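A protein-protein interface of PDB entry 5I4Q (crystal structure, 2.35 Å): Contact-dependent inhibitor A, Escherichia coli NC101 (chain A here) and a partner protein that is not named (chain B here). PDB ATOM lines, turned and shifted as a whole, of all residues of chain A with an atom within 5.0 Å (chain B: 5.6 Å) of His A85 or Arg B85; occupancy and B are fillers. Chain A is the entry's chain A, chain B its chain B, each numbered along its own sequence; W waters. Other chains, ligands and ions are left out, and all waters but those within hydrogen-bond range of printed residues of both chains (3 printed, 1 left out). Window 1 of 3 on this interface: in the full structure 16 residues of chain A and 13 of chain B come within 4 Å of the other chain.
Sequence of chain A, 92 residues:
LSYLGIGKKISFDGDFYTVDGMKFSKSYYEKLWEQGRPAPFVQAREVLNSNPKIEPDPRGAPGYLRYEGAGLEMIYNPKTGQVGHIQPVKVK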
ATOM      1  N   TYR A  28     -31.328  13.182 -24.434  1.00  0.00           N
ATOM      2  CA  TYR A  28     -30.028  12.810 -23.890  1.00  0.00           C
ATOM      3  C   TYR A  28     -29.130  14.054 -23.825  1.00  0.00           C
ATOM      4  O   TYR A  28     -28.506  14.328 -22.798  1.00  0.00           O
ATOM      5  CB  TYR A  28     -29.376  11.657 -24.654  1.00  0.00           C
ATOM      6  CG  TYR A  28     -28.165  11.102 -23.971  1.00  0.00           C
ATOM      7  CD1 TYR A  28     -28.208  10.726 -22.621  1.00  0.00           C
ATOM      8  CD2 TYR A  28     -26.999  10.908 -24.659  1.00  0.00           C
ATOM      9  CE1 TYR A  28     -27.089  10.218 -21.965  1.00  0.00           C
ATOM     10  CE2 TYR A  28     -25.860  10.419 -24.025  1.00  0.00           C
ATOM     11  CZ  TYR A  28     -25.898  10.063 -22.688  1.00  0.00           C
ATOM     12  OH  TYR A  28     -24.755   9.578 -22.088  1.00  0.00           O
ATOM     13  N   ARG A  37     -22.686  17.438 -16.801  1.00  0.00           N
ATOM     14  CA  ARG A  37     -21.745  16.968 -17.816  1.00  0.00           C
ATOM     15  C   ARG A  37     -21.876  17.775 -19.110  1.00  0.00           C
ATOM     16  O   ARG A  37     -22.379  17.280 -20.122  1.00  0.00           O
ATOM     17  CB  ARG A  37     -21.926  15.490 -18.069  1.00  0.00           C
ATOM     18  CG  ARG A  37     -21.395  14.664 -16.896  1.00  0.00           C
ATOM     19  CD  ARG A  37     -22.297  13.505 -16.565  1.00  0.00           C
ATOM     20  NE  ARG A  37     -22.042  12.364 -17.430  1.00  0.00           N
ATOM     21  CZ  ARG A  37     -22.672  11.207 -17.314  1.00  0.00           C
ATOM     22  NH1 ARG A  37     -23.608  11.023 -16.379  1.00  0.00           N
ATOM     23  NH2 ARG A  37     -22.377  10.239 -18.145  1.00  0.00           N
ATOM     24  N   ASP A  57     -20.334  -2.620 -29.708  1.00  0.00           N
ATOM     25  CA  ASP A  57     -21.139  -2.370 -28.503  1.00  0.00           C
ATOM     26  C   ASP A  57     -21.296  -3.671 -27.698  1.00  0.00           C
ATOM     27  O   ASP A  57     -21.884  -4.612 -28.193  1.00  0.00           O
ATOM     28  CB  ASP A  57     -22.501  -1.838 -28.908  1.00  0.00           C
ATOM     29  CG  ASP A  57     -23.428  -1.548 -27.700  1.00  0.00           C
ATOM     30  OD1 ASP A  57     -22.973  -1.654 -26.534  1.00  0.00           O
ATOM     31  OD2 ASP A  57     -24.629  -1.203 -27.934  1.00  0.00           O
ATOM     32  N   ARG A  59     -23.371  -4.340 -25.368  1.00  0.00           N
ATOM     33  CA  ARG A  59     -24.792  -4.618 -25.248  1.00  0.00           C
ATOM     34  C   ARG A  59     -25.452  -4.953 -26.578  1.00  0.00           C
ATOM     35  O   ARG A  59     -26.576  -5.370 -26.589  1.00  0.00           O
ATOM     36  CB  ARG A  59     -25.510  -3.430 -24.614  1.00  0.00           C
ATOM     37  CG  ARG A  59     -24.987  -3.067 -23.224  1.00  0.00           C
ATOM     38  CD  ARG A  59     -24.833  -4.290 -22.327  1.00  0.00           C
ATOM     39  NE  ARG A  59     -24.247  -3.906 -21.049  1.00  0.00           N
ATOM     40  CZ  ARG A  59     -23.163  -4.450 -20.506  1.00  0.00           C
ATOM     41  NH1 ARG A  59     -22.542  -5.458 -21.101  1.00  0.00           N
ATOM     42  NH2 ARG A  59     -22.711  -3.983 -19.345  1.00  0.00           N
ATOM     43  N   ALA A  61     -26.442  -3.041 -29.305  1.00  0.00           N
ATOM     44  CA  ALA A  61     -27.277  -2.134 -30.085  1.00  0.00           C
ATOM     45  C   ALA A  61     -26.808  -2.088 -31.554  1.00  0.00           C
ATOM     46  O   ALA A  61     -25.617  -1.981 -31.812  1.00  0.00           O
ATOM     47  CB  ALA A  61     -27.310  -0.752 -29.495  1.00  0.00           C
ATOM     48  N   GLU A  73     -15.838   6.855 -22.261  1.00  0.00           N
ATOM     49  CA  GLU A  73     -16.363   5.715 -22.979  1.00  0.00           C
ATOM     50  C   GLU A  73     -17.602   6.228 -23.615  1.00  0.00           C
ATOM     51  O   GLU A  73     -18.451   6.898 -22.976  1.00  0.00           O
ATOM     52  CB  GLU A  73     -16.805   4.548 -22.092  1.00  0.00           C
ATOM     53  CG  GLU A  73     -15.728   4.003 -21.166  1.00  0.00           C
ATOM     54  CD  GLU A  73     -16.257   3.071 -20.050  1.00  0.00           C
ATOM     55  OE1 GLU A  73     -17.471   2.780 -20.035  1.00  0.00           O
ATOM     56  OE2 GLU A  73     -15.432   2.641 -19.175  1.00  0.00           O
ATOM     57  N   MET A  74     -17.758   5.831 -24.862  1.00  0.00           N
ATOM     58  CA  MET A  74     -18.848   6.301 -25.663  1.00  0.00           C
ATOM     59  C   MET A  74     -19.390   5.167 -26.510  1.00  0.00           C
ATOM     60  O   MET A  74     -18.643   4.311 -27.019  1.00  0.00           O
ATOM     61  CB  MET A  74     -18.247   7.376 -26.537  1.00  0.00           C
ATOM     62  CG  MET A  74     -19.123   7.690 -27.699  1.00  0.00           C
ATOM     63  SD  MET A  74     -18.395   9.266 -28.603  1.00  0.00           S
ATOM     64  CE  MET A  74     -17.264   8.459 -30.012  1.00  0.00           C
ATOM     65  N   ILE A  75     -20.697   5.200 -26.699  1.00  0.00           N
ATOM     66  CA  ILE A  75     -21.399   4.291 -27.558  1.00  0.00           C
ATOM     67  C   ILE A  75     -21.890   5.180 -28.711  1.00  0.00           C
ATOM     68  O   ILE A  75     -22.693   6.117 -28.514  1.00  0.00           O
ATOM     69  CB  ILE A  75     -22.572   3.650 -26.805  1.00  0.00           C
ATOM     70  CG1 ILE A  75     -22.089   2.924 -25.525  1.00  0.00           C
ATOM     71  CG2 ILE A  75     -23.409   2.730 -27.703  1.00  0.00           C
ATOM     72  CD1 ILE A  75     -21.127   1.770 -25.737  1.00  0.00           C
ATOM     73  N   VAL A  83     -24.196   9.780 -31.075  1.00  0.00           N
ATOM     74  CA  VAL A  83     -23.666   9.414 -29.752  1.00  0.00           C
ATOM     75  C   VAL A  83     -24.799   8.918 -28.889  1.00  0.00           C
ATOM     76  O   VAL A  83     -25.621   9.723 -28.451  1.00  0.00           O
ATOM     77  CB  VAL A  83     -23.066  10.659 -29.063  1.00  0.00           C
ATOM     78  CG1 VAL A  83     -22.543  10.303 -27.695  1.00  0.00           C
ATOM     79  CG2 VAL A  83     -21.967  11.229 -29.921  1.00  0.00           C
ATOM     80  N   GLY A  84     -24.876   7.615 -28.639  1.00  0.00           N
ATOM     81  CA  GLY A  84     -26.018   7.073 -27.864  1.00  0.00           C
ATOM     82  C   GLY A  84     -25.811   7.150 -26.349  1.00  0.00           C
ATOM     83  O   GLY A  84     -26.774   7.195 -25.570  1.00  0.00           O
ATOM     84  N   HIS A  85     -24.540   7.128 -25.951  1.00  0.00           N
ATOM     85  CA  HIS A  85     -24.149   7.204 -24.568  1.00  0.00           C
ATOM     86  C   HIS A  85     -22.667   7.575 -24.424  1.00  0.00           C
ATOM     87  O   HIS A  85     -21.827   7.058 -25.140  1.00  0.00           O
ATOM     88  CB  HIS A  85     -24.404   5.884 -23.889  1.00  0.00           C
ATOM     89  CG  HIS A  85     -24.073   5.892 -22.434  1.00  0.00           C
ATOM     90  ND1 HIS A  85     -22.984   5.229 -21.912  1.00  0.00           N
ATOM     91  CD2 HIS A  85     -24.710   6.470 -21.384  1.00  0.00           C
ATOM     92  CE1 HIS A  85     -22.950   5.416 -20.606  1.00  0.00           C
ATOM     93  NE2 HIS A  85     -23.989   6.164 -20.264  1.00  0.00           N
ATOM     94  N   ILE A  86     -22.374   8.450 -23.467  1.00  0.00           N
ATOM     95  CA  ILE A  86     -21.036   8.869 -23.166  1.00  0.00           C
ATOM     96  C   ILE A  86     -20.951   9.159 -21.639  1.00  0.00           C
ATOM     97  O   ILE A  86     -21.841   9.760 -21.083  1.00  0.00           O
ATOM     98  CB  ILE A  86     -20.658  10.100 -24.002  1.00  0.00           C
ATOM     99  CG1 ILE A  86     -19.217  10.517 -23.760  1.00  0.00           C
ATOM    100  CG2 ILE A  86     -21.597  11.239 -23.736  1.00  0.00           C
ATOM    101  CD1 ILE A  86     -18.595  11.263 -24.939  1.00  0.00           C
ATOM    102  N   GLN A  87     -19.893   8.666 -20.991  1.00  0.00           N
ATOM    103  CA  GLN A  87     -19.623   8.889 -19.563  1.00  0.00           C
ATOM    104  C   GLN A  87     -18.124   8.700 -19.278  1.00  0.00           C
ATOM    105  O   GLN A  87     -17.414   8.086 -20.113  1.00  0.00           O
ATOM    106  CB  GLN A  87     -20.434   7.934 -18.705  1.00  0.00           C
ATOM    107  CG  GLN A  87     -19.926   6.515 -18.648  1.00  0.00           C
ATOM    108  CD  GLN A  87     -20.603   5.683 -17.534  1.00  0.00           C
ATOM    109  OE1 GLN A  87     -20.808   6.135 -16.392  1.00  0.00           O
ATOM    110  NE2 GLN A  87     -20.880   4.473 -17.850  1.00  0.00           N
ATOM    111  N   PHE B  55     -33.187   3.799 -12.862  1.00  0.00           N
ATOM    112  CA  PHE B  55     -32.341   4.767 -13.578  1.00  0.00           C
ATOM    113  C   PHE B  55     -32.540   6.210 -13.184  1.00  0.00           C
ATOM    114  O   PHE B  55     -31.610   7.051 -13.340  1.00  0.00           O
ATOM    115  CB  PHE B  55     -32.501   4.620 -15.091  1.00  0.00           C
ATOM    116  CG  PHE B  55     -31.975   3.319 -15.626  1.00  0.00           C
ATOM    117  CD1 PHE B  55     -30.624   3.068 -15.606  1.00  0.00           C
ATOM    118  CD2 PHE B  55     -32.817   2.387 -16.192  1.00  0.00           C
ATOM    119  CE1 PHE B  55     -30.104   1.898 -16.130  1.00  0.00           C
ATOM    120  CE2 PHE B  55     -32.315   1.179 -16.679  1.00  0.00           C
ATOM    121  CZ  PHE B  55     -30.950   0.948 -16.666  1.00  0.00           C
ATOM    122  N   TYR B  81     -21.541   4.337 -12.305  1.00  0.00           N
ATOM    123  CA  TYR B  81     -20.949   3.928 -13.579  1.00  0.00           C
ATOM    124  C   TYR B  81     -21.790   2.851 -14.287  1.00  0.00           C
ATOM    125  O   TYR B  81     -22.302   3.026 -15.399  1.00  0.00           O
ATOM    126  CB  TYR B  81     -19.510   3.443 -13.350  1.00  0.00           C
ATOM    127  CG  TYR B  81     -18.952   2.798 -14.573  1.00  0.00           C
ATOM    128  CD1 TYR B  81     -18.436   3.574 -15.639  1.00  0.00           C
ATOM    129  CD2 TYR B  81     -18.977   1.416 -14.720  1.00  0.00           C
ATOM    130  CE1 TYR B  81     -17.976   2.977 -16.802  1.00  0.00           C
ATOM    131  CE2 TYR B  81     -18.500   0.819 -15.875  1.00  0.00           C
ATOM    132  CZ  TYR B  81     -18.001   1.602 -16.898  1.00  0.00           C
ATOM    133  OH  TYR B  81     -17.577   0.986 -18.030  1.00  0.00           O
ATOM    134  N   HIS B  82     -21.941   1.712 -13.661  1.00  0.00           N
ATOM    135  CA  HIS B  82     -22.615   0.572 -14.342  1.00  0.00           C
ATOM    136  C   HIS B  82     -24.035   0.831 -14.837  1.00  0.00           C
ATOM    137  O   HIS B  82     -24.427   0.283 -15.861  1.00  0.00           O
ATOM    138  CB  HIS B  82     -22.648  -0.624 -13.427  1.00  0.00           C
ATOM    139  CG  HIS B  82     -21.293  -1.182 -13.129  1.00  0.00           C
ATOM    140  ND1 HIS B  82     -20.524  -1.798 -14.092  1.00  0.00           N
ATOM    141  CD2 HIS B  82     -20.609  -1.295 -11.969  1.00  0.00           C
ATOM    142  CE1 HIS B  82     -19.398  -2.218 -13.544  1.00  0.00           C
ATOM    143  NE2 HIS B  82     -19.431  -1.933 -12.256  1.00  0.00           N
ATOM    144  N   LEU B  83     -24.798   1.664 -14.129  1.00  0.00           N
ATOM    145  CA  LEU B  83     -26.200   1.913 -14.465  1.00  0.00           C
ATOM    146  C   LEU B  83     -26.463   3.215 -15.189  1.00  0.00           C
ATOM    147  O   LEU B  83     -27.608   3.614 -15.346  1.00  0.00           O
ATOM    148  CB  LEU B  83     -27.036   1.871 -13.202  1.00  0.00           C
ATOM    149  CG  LEU B  83     -27.277   0.474 -12.573  1.00  0.00           C
ATOM    150  CD1 LEU B  83     -28.465   0.520 -11.621  1.00  0.00           C
ATOM    151  CD2 LEU B  83     -27.567  -0.596 -13.575  1.00  0.00           C
ATOM    152  N   ASP B  84     -25.422   3.880 -15.646  1.00  0.00           N
ATOM    153  CA  ASP B  84     -25.567   5.150 -16.348  1.00  0.00           C
ATOM    154  C   ASP B  84     -26.308   5.005 -17.659  1.00  0.00           C
ATOM    155  O   ASP B  84     -27.203   5.756 -17.961  1.00  0.00           O
ATOM    156  CB  ASP B  84     -24.183   5.772 -16.641  1.00  0.00           C
ATOM    157  CG  ASP B  84     -24.291   7.218 -17.014  1.00  0.00           C
ATOM    158  OD1 ASP B  84     -24.686   8.019 -16.142  1.00  0.00           O
ATOM    159  OD2 ASP B  84     -24.101   7.568 -18.173  1.00  0.00           O
ATOM    160  N   ARG B  85     -25.936   4.012 -18.434  1.00  0.00           N
ATOM    161  CA  ARG B  85     -26.555   3.798 -19.706  1.00  0.00           C
ATOM    162  C   ARG B  85     -27.935   3.130 -19.523  1.00  0.00           C
ATOM    163  O   ARG B  85     -28.030   2.051 -18.967  1.00  0.00           O
ATOM    164  CB  ARG B  85     -25.638   2.911 -20.537  1.00  0.00           C
ATOM    165  CG  ARG B  85     -26.182   2.671 -21.945  1.00  0.00           C
ATOM    166  CD  ARG B  85     -25.277   1.766 -22.792  1.00  0.00           C
ATOM    167  NE  ARG B  85     -25.935   1.390 -24.075  1.00  0.00           N
ATOM    168  CZ  ARG B  85     -25.415   0.576 -24.969  1.00  0.00           C
ATOM    169  NH1 ARG B  85     -24.263  -0.029 -24.702  1.00  0.00           N
ATOM    170  NH2 ARG B  85     -26.099   0.309 -26.084  1.00  0.00           N
ATOM    171  N   ASP B  86     -28.964   3.785 -20.047  1.00  0.00           N
ATOM    172  CA  ASP B  86     -30.336   3.420 -19.909  1.00  0.00           C
ATOM    173  C   ASP B  86     -30.967   3.335 -21.285  1.00  0.00           C
ATOM    174  O   ASP B  86     -31.346   4.337 -21.861  1.00  0.00           O
ATOM    175  CB  ASP B  86     -31.037   4.485 -19.044  1.00  0.00           C
ATOM    176  CG  ASP B  86     -32.583   4.326 -18.976  1.00  0.00           C
ATOM    177  OD1 ASP B  86     -33.133   3.259 -19.349  1.00  0.00           O
ATOM    178  OD2 ASP B  86     -33.238   5.299 -18.531  1.00  0.00           O
ATOM    179  N   ASP B  87     -31.033   2.122 -21.839  1.00  0.00           N
ATOM    180  CA  ASP B  87     -31.786   1.907 -23.047  1.00  0.00           C
ATOM    181  C   ASP B  87     -32.264   0.461 -23.059  1.00  0.00           C
ATOM    182  O   ASP B  87     -31.989  -0.288 -22.126  1.00  0.00           O
ATOM    183  CB  ASP B  87     -30.909   2.216 -24.293  1.00  0.00           C
ATOM    184  CG  ASP B  87     -29.611   1.428 -24.296  1.00  0.00           C
ATOM    185  OD1 ASP B  87     -29.635   0.207 -23.972  1.00  0.00           O
ATOM    186  OD2 ASP B  87     -28.549   2.021 -24.607  1.00  0.00           O
ATOM    187  N   TYR B  89     -31.171  -2.117 -24.630  1.00  0.00           N
ATOM    188  CA  TYR B  89     -30.094  -3.096 -24.698  1.00  0.00           C
ATOM    189  C   TYR B  89     -29.415  -3.248 -23.366  1.00  0.00           C
ATOM    190  O   TYR B  89     -29.019  -4.357 -23.011  1.00  0.00           O
ATOM    191  CB  TYR B  89     -29.102  -2.773 -25.849  1.00  0.00           C
ATOM    192  CG  TYR B  89     -29.801  -2.790 -27.188  1.00  0.00           C
ATOM    193  CD1 TYR B  89     -30.044  -3.998 -27.844  1.00  0.00           C
ATOM    194  CD2 TYR B  89     -30.280  -1.612 -27.762  1.00  0.00           C
ATOM    195  CE1 TYR B  89     -30.721  -4.040 -29.036  1.00  0.00           C
ATOM    196  CE2 TYR B  89     -30.961  -1.629 -28.948  1.00  0.00           C
ATOM    197  CZ  TYR B  89     -31.196  -2.848 -29.588  1.00  0.00           C
ATOM    198  OH  TYR B  89     -31.882  -2.855 -30.812  1.00  0.00           O
ATOM    199  N   SER B  90     -29.307  -2.164 -22.602  1.00  0.00           N
ATOM    200  CA  SER B  90     -28.738  -2.271 -21.253  1.00  0.00           C
ATOM    201  C   SER B  90     -29.778  -2.895 -20.331  1.00  0.00           C
ATOM    202  O   SER B  90     -29.444  -3.691 -19.456  1.00  0.00           O
ATOM    203  CB  SER B  90     -28.255  -0.914 -20.733  1.00  0.00           C
ATOM    204  OG  SER B  90     -29.339  -0.062 -20.337  1.00  0.00           O
ATOM    205  N   TRP B  94     -29.238  -6.123 -17.909  1.00  0.00           N
ATOM    206  CA  TRP B  94     -29.372  -6.061 -16.444  1.00  0.00           C
ATOM    207  C   TRP B  94     -30.498  -6.953 -15.982  1.00  0.00           C
ATOM    208  O   TRP B  94     -30.369  -7.616 -14.954  1.00  0.00           O
ATOM    209  CB  TRP B  94     -29.536  -4.617 -15.960  1.00  0.00           C
ATOM    210  CG  TRP B  94     -28.254  -3.803 -16.101  1.00  0.00           C
ATOM    211  CD1 TRP B  94     -28.087  -2.669 -16.844  1.00  0.00           C
ATOM    212  CD2 TRP B  94     -26.986  -4.075 -15.493  1.00  0.00           C
ATOM    213  NE1 TRP B  94     -26.790  -2.224 -16.742  1.00  0.00           N
ATOM    214  CE2 TRP B  94     -26.093  -3.074 -15.918  1.00  0.00           C
ATOM    215  CE3 TRP B  94     -26.520  -5.068 -14.644  1.00  0.00           C
ATOM    216  CZ2 TRP B  94     -24.737  -3.057 -15.543  1.00  0.00           C
ATOM    217  CZ3 TRP B  94     -25.179  -5.045 -14.249  1.00  0.00           C
ATOM    218  CH2 TRP B  94     -24.312  -4.037 -14.688  1.00  0.00           C
HETATM  219  O   HOH W   1     -28.242  -6.195 -24.789  1.00  0.00           O
HETATM  220  O   HOH W   2     -21.572  -1.761 -16.961  1.00  0.00           O
HETATM  221  O   HOH W   3     -24.987   9.467 -19.588  1.00  0.00           O
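The backbone NH of Arg B85 lies within hydrogen-bond range of a ring nitrogen (NE2) of His A85 (3.4 Å). The side-chain carboxylate (OD1) of Asp A57 is in salt-bridge range of the guanidinium group (NH1) of Arg B85. The backbone carbonyl oxygen of Tyr B81 sits at hydrogen-bond distance from the side-chain amide nitrogen of Gln A87, at 3.2 Å. OH of Tyr B81 is in hydrogen-bond range of OE1 of Glu A73 (2.7 Å). OD2 of Asp B84 is in hydrogen-bond range of NE2 of His A85. The guanidinium group of Arg A37 lies within salt-bridge range of the side-chain carboxylate of Asp B84.
OD1 of Asp B87 lies within hydrogen-bond range of N of Tyr B89, at 2.9 Å. N of Glu A73 sits at hydrogen-bond distance from O of Gln A87 (2.9 Å). O of Ile A75 lies within hydrogen-bond range of N of Gly A84 (2.7 Å). The side-chain carboxylate (OD1) of Asp A57 sits at hydrogen-bond distance from the backbone NH (N) of Arg A59 (3.0 Å). The backbone carbonyl oxygen (O) of His A85 sits at hydrogen-bond distance from the backbone NH (N) of Ile A75 (2.7 Å). NE of Arg B85 lies within salt-bridge range of OD2 of Asp B87 (2.7 Å).
Among the printed residues, merely in contact across the chains: Gln A87 with Asp B84 (3.4 Å), Arg A59 with Arg B85 (3.5 Å), Ala A61 with Tyr B89 (3.5 Å), Arg A59 with Tyr B89 (3.7 Å), Ile A75 with Arg B85 (3.8 Å) and Ala A61 with Arg B85 (3.8 Å).
His A85 touches two residues of chain B. Arg B85 touches just these residues of chain A: Asp A57, Arg A59, Ala A61, Ile A75 and His A85. Printed residues of chain A within 4 Å of Tyr B89: Arg A59 (3.7 Å) and Ala A61 (3.5 Å). Of the printed residues of chain B, Arg A37 touches Asp B84 (3.2 Å). Of the printed residues of chain A, Asp B84 touches Arg A37, His A85 and Gln A87. Of the printed residues of chain B, Arg A59 touches Arg B85 (3.5 Å) and Tyr B89 (3.7 Å). Of the printed residues of chain B, Glu A73 touches Tyr B81 (2.7 Å). Phe B55 touches none of the printed residues of chain A. Trp B94 touches none of the printed residues of chain A. The nearest residue of chain B that does not touch His A85 is Asp B86 (5.2 Å).
Hydrophobic or aromatic side chains of chain B that line the printed part of chain A: Tyr B81 and Tyr B89. Of the 13 printed residues of chain A, 8 touch a printed residue of chain B.
Water W3 lies within hydrogen-bond range of OH of Tyr A28, OD2 of Asp B84, NH2 of Arg A37 and O of Ile A86. Water W1 lies within hydrogen-bond range of O of Arg A59 (2.6 Å) and O of Tyr B89 (2.7 Å). Water W2 lies within hydrogen-bond range of ND1 of His B82 (3.1 Å) and NH2 of Arg A59 (3.5 Å).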
